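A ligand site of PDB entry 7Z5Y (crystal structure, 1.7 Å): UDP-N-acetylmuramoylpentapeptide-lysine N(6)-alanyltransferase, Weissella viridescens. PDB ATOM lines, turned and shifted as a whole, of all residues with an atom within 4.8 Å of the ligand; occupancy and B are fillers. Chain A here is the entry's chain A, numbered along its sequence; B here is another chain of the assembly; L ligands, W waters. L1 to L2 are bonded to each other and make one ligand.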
ATOM      1  N   LYS A  37       2.401  16.340  -2.248  1.00  0.00           N
ATOM      2  CA  LYS A  37       3.244  17.533  -2.354  1.00  0.00           C
ATOM      3  C   LYS A  37       2.413  18.747  -2.775  1.00  0.00           C
ATOM      4  O   LYS A  37       2.668  19.380  -3.804  1.00  0.00           O
ATOM      5  CB  LYS A  37       4.370  17.290  -3.342  1.00  0.00           C
ATOM      6  CG  LYS A  37       5.240  16.085  -3.031  1.00  0.00           C
ATOM      7  CD  LYS A  37       6.194  16.362  -1.891  1.00  0.00           C
ATOM      8  CE  LYS A  37       7.250  15.276  -1.812  1.00  0.00           C
ATOM      9  NZ  LYS A  37       7.961  15.320  -0.507  1.00  0.00           N
ATOM     10  N   ASN A  39       2.182  21.733  -1.840  1.00  0.00           N
ATOM     11  CA  ASN A  39       2.887  23.008  -1.957  1.00  0.00           C
ATOM     12  C   ASN A  39       3.759  23.131  -3.212  1.00  0.00           C
ATOM     13  O   ASN A  39       4.447  24.150  -3.378  1.00  0.00           O
ATOM     14  CB  ASN A  39       3.746  23.234  -0.694  1.00  0.00           C
ATOM     15  CG  ASN A  39       4.679  22.053  -0.384  1.00  0.00           C
ATOM     16  OD1 ASN A  39       4.324  20.884  -0.573  1.00  0.00           O
ATOM     17  ND2 ASN A  39       5.881  22.367   0.090  1.00  0.00           N
ATOM     18  N   TRP A  40       3.759  22.130  -4.110  1.00  0.00           N
ATOM     19  CA  TRP A  40       4.515  22.161  -5.360  1.00  0.00           C
ATOM     20  C   TRP A  40       3.554  22.246  -6.540  1.00  0.00           C
ATOM     21  O   TRP A  40       2.380  21.880  -6.438  1.00  0.00           O
ATOM     22  CB  TRP A  40       5.412  20.921  -5.509  1.00  0.00           C
ATOM     23  CG  TRP A  40       6.501  20.825  -4.477  1.00  0.00           C
ATOM     24  CD1 TRP A  40       6.351  20.699  -3.130  1.00  0.00           C
ATOM     25  CD2 TRP A  40       7.911  20.793  -4.732  1.00  0.00           C
ATOM     26  NE1 TRP A  40       7.586  20.621  -2.507  1.00  0.00           N
ATOM     27  CE2 TRP A  40       8.560  20.664  -3.478  1.00  0.00           C
ATOM     28  CE3 TRP A  40       8.687  20.852  -5.893  1.00  0.00           C
ATOM     29  CZ2 TRP A  40       9.950  20.617  -3.350  1.00  0.00           C
ATOM     30  CZ3 TRP A  40      10.079  20.791  -5.770  1.00  0.00           C
ATOM     31  CH2 TRP A  40      10.692  20.684  -4.505  1.00  0.00           C
ATOM     32  N   ASP A  64       9.727  26.453  -5.400  1.00  0.00           N
ATOM     33  CA  ASP A  64      10.248  27.805  -5.364  1.00  0.00           C
ATOM     34  C   ASP A  64      11.710  27.802  -4.936  1.00  0.00           C
ATOM     35  O   ASP A  64      12.203  26.859  -4.308  1.00  0.00           O
ATOM     36  CB  ASP A  64       9.406  28.668  -4.421  1.00  0.00           C
ATOM     37  CG  ASP A  64       8.131  29.179  -5.087  1.00  0.00           C
ATOM     38  OD1 ASP A  64       7.031  28.819  -4.626  1.00  0.00           O
ATOM     39  OD2 ASP A  64       8.246  29.898  -6.119  1.00  0.00           O
ATOM     40  N   THR A  65      12.408  28.864  -5.312  1.00  0.00           N
ATOM     41  CA  THR A  65      13.815  29.079  -4.984  1.00  0.00           C
ATOM     42  C   THR A  65      13.994  30.536  -4.596  1.00  0.00           C
ATOM     43  O   THR A  65      13.088  31.356  -4.834  1.00  0.00           O
ATOM     44  CB  THR A  65      14.738  28.748  -6.168  1.00  0.00           C
ATOM     45  OG1 THR A  65      14.733  29.867  -7.077  1.00  0.00           O
ATOM     46  CG2 THR A  65      14.323  27.464  -6.892  1.00  0.00           C
ATOM     47  N   PHE A  71      12.477  25.317  -9.422  1.00  0.00           N
ATOM     48  CA  PHE A  71      13.220  24.075  -9.436  1.00  0.00           C
ATOM     49  C   PHE A  71      12.223  22.989  -9.827  1.00  0.00           C
ATOM     50  O   PHE A  71      11.181  22.860  -9.193  1.00  0.00           O
ATOM     51  CB  PHE A  71      13.844  23.813  -8.072  1.00  0.00           C
ATOM     52  CG  PHE A  71      14.269  22.390  -7.835  1.00  0.00           C
ATOM     53  CD1 PHE A  71      15.345  21.835  -8.509  1.00  0.00           C
ATOM     54  CD2 PHE A  71      13.613  21.616  -6.892  1.00  0.00           C
ATOM     55  CE1 PHE A  71      15.742  20.510  -8.263  1.00  0.00           C
ATOM     56  CE2 PHE A  71      14.014  20.300  -6.626  1.00  0.00           C
ATOM     57  CZ  PHE A  71      15.077  19.758  -7.324  1.00  0.00           C
ATOM     58  N   TYR A  73      11.352  19.028 -10.511  1.00  0.00           N
ATOM     59  CA  TYR A  73      11.872  17.790  -9.931  1.00  0.00           C
ATOM     60  C   TYR A  73      10.936  16.622 -10.220  1.00  0.00           C
ATOM     61  O   TYR A  73       9.757  16.670  -9.839  1.00  0.00           O
ATOM     62  CB  TYR A  73      12.107  17.979  -8.441  1.00  0.00           C
ATOM     63  CG  TYR A  73      12.533  16.727  -7.685  1.00  0.00           C
ATOM     64  CD1 TYR A  73      13.544  15.916  -8.188  1.00  0.00           C
ATOM     65  CD2 TYR A  73      11.998  16.428  -6.438  1.00  0.00           C
ATOM     66  CE1 TYR A  73      13.976  14.780  -7.492  1.00  0.00           C
ATOM     67  CE2 TYR A  73      12.406  15.278  -5.731  1.00  0.00           C
ATOM     68  CZ  TYR A  73      13.411  14.472  -6.274  1.00  0.00           C
ATOM     69  OH  TYR A  73      13.843  13.344  -5.607  1.00  0.00           O
ATOM     70  N   TYR A 104      14.981  26.602 -13.669  1.00  0.00           N
ATOM     71  CA  TYR A 104      16.401  26.663 -13.958  1.00  0.00           C
ATOM     72  C   TYR A 104      16.999  25.280 -14.238  1.00  0.00           C
ATOM     73  O   TYR A 104      18.067  25.195 -14.868  1.00  0.00           O
ATOM     74  CB  TYR A 104      17.151  27.351 -12.815  1.00  0.00           C
ATOM     75  CG  TYR A 104      17.395  26.509 -11.559  1.00  0.00           C
ATOM     76  CD1 TYR A 104      18.563  25.754 -11.435  1.00  0.00           C
ATOM     77  CD2 TYR A 104      16.496  26.531 -10.475  1.00  0.00           C
ATOM     78  CE1 TYR A 104      18.836  24.997 -10.297  1.00  0.00           C
ATOM     79  CE2 TYR A 104      16.749  25.757  -9.311  1.00  0.00           C
ATOM     80  CZ  TYR A 104      17.934  25.010  -9.233  1.00  0.00           C
ATOM     81  OH  TYR A 104      18.240  24.245  -8.126  1.00  0.00           O
ATOM     82  N   ARG A 107      15.466  18.118 -12.724  1.00  0.00           N
ATOM     83  CA  ARG A 107      16.215  17.057 -12.057  1.00  0.00           C
ATOM     84  C   ARG A 107      15.379  15.787 -11.991  1.00  0.00           C
ATOM     85  O   ARG A 107      14.211  15.836 -11.583  1.00  0.00           O
ATOM     86  CB  ARG A 107      16.633  17.461 -10.648  1.00  0.00           C
ATOM     87  CG  ARG A 107      17.220  16.306  -9.849  1.00  0.00           C
ATOM     88  CD  ARG A 107      17.812  16.843  -8.577  1.00  0.00           C
ATOM     89  NE  ARG A 107      18.907  17.769  -8.864  1.00  0.00           N
ATOM     90  CZ  ARG A 107      19.426  18.600  -7.979  1.00  0.00           C
ATOM     91  NH1 ARG A 107      18.930  18.701  -6.751  1.00  0.00           N
ATOM     92  NH2 ARG A 107      20.461  19.362  -8.320  1.00  0.00           N
ATOM     93  N   ILE A 143      18.849  14.658  -2.871  1.00  0.00           N
ATOM     94  CA  ILE A 143      17.537  14.768  -2.215  1.00  0.00           C
ATOM     95  C   ILE A 143      17.116  13.416  -1.640  1.00  0.00           C
ATOM     96  O   ILE A 143      16.788  13.306  -0.451  1.00  0.00           O
ATOM     97  CB  ILE A 143      16.484  15.305  -3.206  1.00  0.00           C
ATOM     98  CG1 ILE A 143      16.818  16.727  -3.660  1.00  0.00           C
ATOM     99  CG2 ILE A 143      15.104  15.252  -2.584  1.00  0.00           C
ATOM    100  CD1 ILE A 143      15.947  17.186  -4.827  1.00  0.00           C
ATOM    101  N   THR A 210      14.038  16.506  12.090  1.00  0.00           N
ATOM    102  CA  THR A 210      12.834  17.186  11.658  1.00  0.00           C
ATOM    103  C   THR A 210      11.789  16.188  11.155  1.00  0.00           C
ATOM    104  O   THR A 210      12.118  15.061  10.745  1.00  0.00           O
ATOM    105  CB  THR A 210      13.174  18.237  10.593  1.00  0.00           C
ATOM    106  OG1 THR A 210      13.783  17.612   9.448  1.00  0.00           O
ATOM    107  CG2 THR A 210      14.137  19.283  11.171  1.00  0.00           C
ATOM    108  N   HIS A 211      10.521  16.598  11.190  1.00  0.00           N
ATOM    109  CA  HIS A 211       9.407  15.694  10.933  1.00  0.00           C
ATOM    110  C   HIS A 211       8.259  16.436  10.251  1.00  0.00           C
ATOM    111  O   HIS A 211       8.038  17.636  10.472  1.00  0.00           O
ATOM    112  CB  HIS A 211       8.949  15.031  12.237  1.00  0.00           C
ATOM    113  CG  HIS A 211       8.388  15.988  13.248  1.00  0.00           C
ATOM    114  ND1 HIS A 211       7.088  15.935  13.708  1.00  0.00           N
ATOM    115  CD2 HIS A 211       8.960  17.037  13.880  1.00  0.00           C
ATOM    116  CE1 HIS A 211       6.891  16.891  14.593  1.00  0.00           C
ATOM    117  NE2 HIS A 211       8.008  17.584  14.713  1.00  0.00           N
ATOM    118  N   ARG A 212       7.515  15.698   9.423  1.00  0.00           N
ATOM    119  CA  ARG A 212       6.443  16.275   8.631  1.00  0.00           C
ATOM    120  C   ARG A 212       5.141  16.378   9.438  1.00  0.00           C
ATOM    121  O   ARG A 212       4.895  15.570  10.337  1.00  0.00           O
ATOM    122  CB  ARG A 212       6.214  15.439   7.380  1.00  0.00           C
ATOM    123  CG  ARG A 212       7.474  15.196   6.525  1.00  0.00           C
ATOM    124  CD  ARG A 212       7.118  14.504   5.233  1.00  0.00           C
ATOM    125  NE  ARG A 212       8.254  14.302   4.334  1.00  0.00           N
ATOM    126  CZ  ARG A 212       8.642  15.181   3.414  1.00  0.00           C
ATOM    127  NH1 ARG A 212       8.016  16.322   3.228  1.00  0.00           N
ATOM    128  NH2 ARG A 212       9.676  14.870   2.630  1.00  0.00           N
ATOM    129  N   PRO A 213       4.308  17.378   9.130  1.00  0.00           N
ATOM    130  CA  PRO A 213       3.024  17.503   9.824  1.00  0.00           C
ATOM    131  C   PRO A 213       2.075  16.365   9.455  1.00  0.00           C
ATOM    132  O   PRO A 213       2.256  15.685   8.441  1.00  0.00           O
ATOM    133  CB  PRO A 213       2.492  18.862   9.330  1.00  0.00           C
ATOM    134  CG  PRO A 213       3.177  19.102   8.051  1.00  0.00           C
ATOM    135  CD  PRO A 213       4.542  18.476   8.179  1.00  0.00           C
ATOM    136  N   TYR A 216       0.450  15.942   5.899  1.00  0.00           N
ATOM    137  CA  TYR A 216       1.194  15.276   4.825  1.00  0.00           C
ATOM    138  C   TYR A 216       0.720  13.835   4.665  1.00  0.00           C
ATOM    139  O   TYR A 216       0.398  13.382   3.556  1.00  0.00           O
ATOM    140  CB  TYR A 216       2.680  15.300   5.154  1.00  0.00           C
ATOM    141  CG  TYR A 216       3.599  14.831   4.053  1.00  0.00           C
ATOM    142  CD1 TYR A 216       4.103  15.726   3.108  1.00  0.00           C
ATOM    143  CD2 TYR A 216       4.003  13.499   3.983  1.00  0.00           C
ATOM    144  CE1 TYR A 216       4.978  15.283   2.096  1.00  0.00           C
ATOM    145  CE2 TYR A 216       4.869  13.056   2.968  1.00  0.00           C
ATOM    146  CZ  TYR A 216       5.357  13.960   2.036  1.00  0.00           C
ATOM    147  OH  TYR A 216       6.205  13.539   1.039  1.00  0.00           O
ATOM    148  N   LEU A 333      22.943  27.959  -7.380  1.00  0.00           N
ATOM    149  CA  LEU A 333      22.189  27.138  -6.425  1.00  0.00           C
ATOM    150  C   LEU A 333      22.726  25.731  -6.238  1.00  0.00           C
ATOM    151  O   LEU A 333      22.348  25.086  -5.248  1.00  0.00           O
ATOM    152  CB  LEU A 333      20.720  27.051  -6.856  1.00  0.00           C
ATOM    153  CG  LEU A 333      19.973  28.382  -6.867  1.00  0.00           C
ATOM    154  CD1 LEU A 333      18.513  28.228  -7.319  1.00  0.00           C
ATOM    155  CD2 LEU A 333      20.041  29.005  -5.479  1.00  0.00           C
ATOM    156  N   ALA B   1      13.794  17.695   6.268  1.00  0.00           N
ATOM    157  CA  ALA B   1      15.219  17.779   5.934  1.00  0.00           C
ATOM    158  C   ALA B   1      15.977  16.573   6.466  1.00  0.00           C
ATOM    159  O   ALA B   1      16.984  16.151   5.886  1.00  0.00           O
ATOM    160  CB  ALA B   1      15.804  19.074   6.476  1.00  0.00           C
ATOM    161  N   FGA B   2      15.498  16.025   7.582  1.00  0.00           N
ATOM    162  CA  FGA B   2      16.151  14.870   8.167  1.00  0.00           C
ATOM    163  C   FGA B   2      16.973  15.252   9.369  1.00  0.00           C
ATOM    164  O   FGA B   2      16.609  16.162  10.132  1.00  0.00           O
ATOM    165  CB  FGA B   2      15.078  13.839   8.518  1.00  0.00           C
ATOM    166  CG  FGA B   2      14.396  13.322   7.262  1.00  0.00           C
ATOM    167  CD  FGA B   2      15.243  12.300   6.524  1.00  0.00           C
ATOM    168  OE1 FGA B   2      16.468  12.358   6.451  1.00  0.00           O
ATOM    169  OXT FGA B   2      18.115  14.604   9.617  1.00  0.00           O
ATOM    170  N   CYS B   3      14.341  12.087   5.441  1.00  0.00           N
ATOM    171  CA  CYS B   3      15.075  11.102   4.630  1.00  0.00           C
ATOM    172  C   CYS B   3      14.530  11.079   3.185  1.00  0.00           C
ATOM    173  O   CYS B   3      14.321  10.017   2.611  1.00  0.00           O
ATOM    174  CB  CYS B   3      14.983   9.723   5.295  1.00  0.00           C
ATOM    175  SG  CYS B   3      16.330   8.591   4.922  1.00  0.00           S
ATOM    176  N   DAL B   4      14.300  12.253   2.605  1.00  0.00           N
ATOM    177  CA  DAL B   4      13.599  12.330   1.322  1.00  0.00           C
ATOM    178  CB  DAL B   4      13.720  13.715   0.725  1.00  0.00           C
ATOM    179  C   DAL B   4      12.121  11.944   1.476  1.00  0.00           C
ATOM    180  O   DAL B   4      11.465  12.334   2.444  1.00  0.00           O
ATOM    181  N   DAL B   5      11.599  11.183   0.505  1.00  0.00           N
ATOM    182  CA  DAL B   5      10.210  10.727   0.563  1.00  0.00           C
ATOM    183  CB  DAL B   5       9.913   9.783  -0.608  1.00  0.00           C
ATOM    184  C   DAL B   5       9.175  11.868   0.630  1.00  0.00           C
ATOM    185  O   DAL B   5       8.146  11.740   1.316  1.00  0.00           O
ATOM    186  OXT DAL B   5       9.326  12.931   0.000  1.00  0.00           O
HETATM  187  C1  LIG L   1      10.332  20.163   2.739  1.00  0.00           C
HETATM  188  C2  LIG L   1      11.159  19.452   3.809  1.00  0.00           C
HETATM  189  C3  LIG L   1      10.225  18.895   4.890  1.00  0.00           C
HETATM  190  C4  LIG L   1       9.247  19.957   5.367  1.00  0.00           C
HETATM  191  C5  LIG L   1       8.465  20.471   4.155  1.00  0.00           C
HETATM  192  C6  LIG L   1       7.408  21.502   4.499  1.00  0.00           C
HETATM  193  C7  LIG L   1      13.244  18.518   2.903  1.00  0.00           C
HETATM  194  C8  LIG L   1      13.892  17.379   2.166  1.00  0.00           C
HETATM  195  C9  LIG L   1      11.356  17.015   5.922  1.00  0.00           C
HETATM  196  C10 LIG L   1      12.848  16.793   5.691  1.00  0.00           C
HETATM  197  C11 LIG L   1      10.886  16.388   7.226  1.00  0.00           C
HETATM  198  O1  LIG L   1       9.563  19.162   2.149  1.00  0.00           O
HETATM  199  O2  LIG L   1      11.030  18.407   5.976  1.00  0.00           O
HETATM  200  O3  LIG L   1       8.317  19.413   6.287  1.00  0.00           O
HETATM  201  O4  LIG L   1       9.397  21.091   3.254  1.00  0.00           O
HETATM  202  O5  LIG L   1       8.001  22.738   4.850  1.00  0.00           O
HETATM  203  O6  LIG L   1      13.883  19.505   3.261  1.00  0.00           O
HETATM  204  O7  LIG L   1      13.192  15.785   5.021  1.00  0.00           O
HETATM  205  N1  LIG L   1      11.926  18.410   3.148  1.00  0.00           N
HETATM  206  N1  LG2 L   2      15.845  21.485  -3.589  1.00  0.00           N
HETATM  207  C1  LG2 L   2      16.941  21.399  -4.446  1.00  0.00           C
HETATM  208  N2  LG2 L   2      17.087  22.478  -5.300  1.00  0.00           N
HETATM  209  C2  LG2 L   2      16.267  23.583  -5.385  1.00  0.00           C
HETATM  210  C3  LG2 L   2      15.163  23.598  -4.469  1.00  0.00           C
HETATM  211  C4  LG2 L   2      14.996  22.563  -3.622  1.00  0.00           C
HETATM  212  O1  LG2 L   2      17.718  20.453  -4.462  1.00  0.00           O
HETATM  213  O2  LG2 L   2      16.522  24.472  -6.229  1.00  0.00           O
HETATM  214  C5  LG2 L   2      15.654  20.393  -2.613  1.00  0.00           C
HETATM  215  C6  LG2 L   2      15.387  20.886  -1.197  1.00  0.00           C
HETATM  216  O3  LG2 L   2      16.586  21.308  -0.544  1.00  0.00           O
HETATM  217  C7  LG2 L   2      14.789  19.623  -0.581  1.00  0.00           C
HETATM  218  C8  LG2 L   2      14.085  18.955  -1.764  1.00  0.00           C
HETATM  219  O4  LG2 L   2      14.502  19.666  -2.955  1.00  0.00           O
HETATM  220  O5  LG2 L   2      15.799  18.737  -0.124  1.00  0.00           O
HETATM  221  C9  LG2 L   2      12.581  18.952  -1.658  1.00  0.00           C
HETATM  222  O6  LG2 L   2      12.260  18.054  -0.571  1.00  0.00           O
HETATM  223  P1  LG2 L   2      10.820  17.449  -0.417  1.00  0.00           P
HETATM  224  O7  LG2 L   2      10.515  16.723  -1.672  1.00  0.00           O
HETATM  225  O8  LG2 L   2      10.706  16.671   0.886  1.00  0.00           O
HETATM  226  O9  LG2 L   2       9.869  18.750  -0.273  1.00  0.00           O
HETATM  227  P2  LG2 L   2       8.766  19.107   0.819  1.00  0.00           P
HETATM  228  O10 LG2 L   2       7.765  17.965   0.682  1.00  0.00           O
HETATM  229  O11 LG2 L   2       8.121  20.373   0.260  1.00  0.00           O
HETATM  230  O   HOH W   1      10.959  14.023  -1.737  1.00  0.00           O
HETATM  231  O   HOH W   2       5.087  18.782   0.821  1.00  0.00           O
HETATM  232  O   HOH W   3      12.061  13.240   4.976  1.00  0.00           O
HETATM  233  O   HOH W   4       6.229  17.790   5.011  1.00  0.00           O
HETATM  234  O   HOH W   5      15.666  14.446   3.713  1.00  0.00           O
HETATM  235  O   HOH W   6       9.351  17.214  -3.861  1.00  0.00           O
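N of FGA 2 of chain B sits at hydrogen-bond distance from the side-chain hydroxyl (OG1) of Thr 210.
OH of Tyr 216 lies within hydrogen-bond range of NZ of Lys 37, at 2.9 Å.
The side-chain amino group (NZ) of Lys 37 is in salt-bridge range of OXT of DAL 5 of chain B (2.8 Å).
OXT of DAL 5 of chain B is in salt-bridge range of the guanidinium group (NH2) of Arg 212.
N of Ala 1 of chain B is in hydrogen-bond range of OG1 of Thr 210.
The guanidinium group (NH2) of Arg 212 lies within hydrogen-bond range of O of DAL 4 of chain B (3.1 Å).
The guanidinium group (NH2) of Arg 212 is in salt-bridge range of an oxygen (O8) of LG2 L2.
OH of Tyr 104 sits at hydrogen-bond distance from O2 of LG2 L2, at 2.6 Å.
The side-chain amino group (NZ) of Lys 37 lies within salt-bridge range of an oxygen (O10) of LG2 L2, 2.9 Å away.
N of Ala 1 of chain B is bonded to C10 of LIG L1.
ND2 of Asn 39 is in hydrogen-bond range of O11 of LG2 L2 (3.0 Å).
O1 of LG2 L2 lies within hydrogen-bond range of NH1 of Arg 107 (3.1 Å).
An oxygen (O11) of LG2 L2 sits at hydrogen-bond distance from the indole nitrogen (NE1) of Trp 40 (2.8 Å).
N of FGA 2 of chain B sits close to an oxygen (O7) of LIG L1 (3.5 Å).
Residues that only touch the ligand: Thr 65 (3.8 Å), Phe 71 (3.3 Å), Ile 143 (3.4 Å), Thr 210 (3.9 Å), His 211 (3.99 Å), Cys 3 of chain B (3.9 Å) and DAL 4 of chain B (3.9 Å).
Hydrophobic or aromatic side chains within 4 Å of the ligand: Trp 40, Phe 71, Tyr 104, Ile 143 and Ala 1 of chain B.
15 residues have an atom within 4 Å of the ligand: Lys 37, Asn 39, Trp 40, Thr 65, Phe 71, Tyr 104, Arg 107, Ile 143, Thr 210, His 211, Arg 212, Ala 1 of chain B, FGA 2 of chain B, Cys 3 of chain B and DAL 4 of chain B.
Water W1 lies within hydrogen-bond range of OXT of DAL 5 of chain B (2.6 Å), an oxygen (O7) of LG2 L2 (2.7 Å) and the side-chain amino group (NZ) of Lys 37 (3.5 Å).
Water W3 lies within hydrogen-bond range of the backbone NH of Cys 3 of chain B (2.6 Å), O of DAL 4 of chain B (2.8 Å) and an oxygen (O7) of LIG L1 (2.8 Å).
Water W2 lies within hydrogen-bond range of the side-chain amide oxygen of Asn 39 and an oxygen (O10) of LG2 L2.
Water W4 bridges the guanidinium group of Arg 212 and an oxygen (O3) of LIG L1.
Water W5 lies within hydrogen-bond range of N of DAL 4 of chain B (2.8 Å), the backbone carbonyl oxygen (O) of Ala 1 of chain B (3.1 Å), an oxygen (O7) of LIG L1 (3.1 Å) and the backbone NH (N) of Cys 3 of chain B (3.2 Å).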
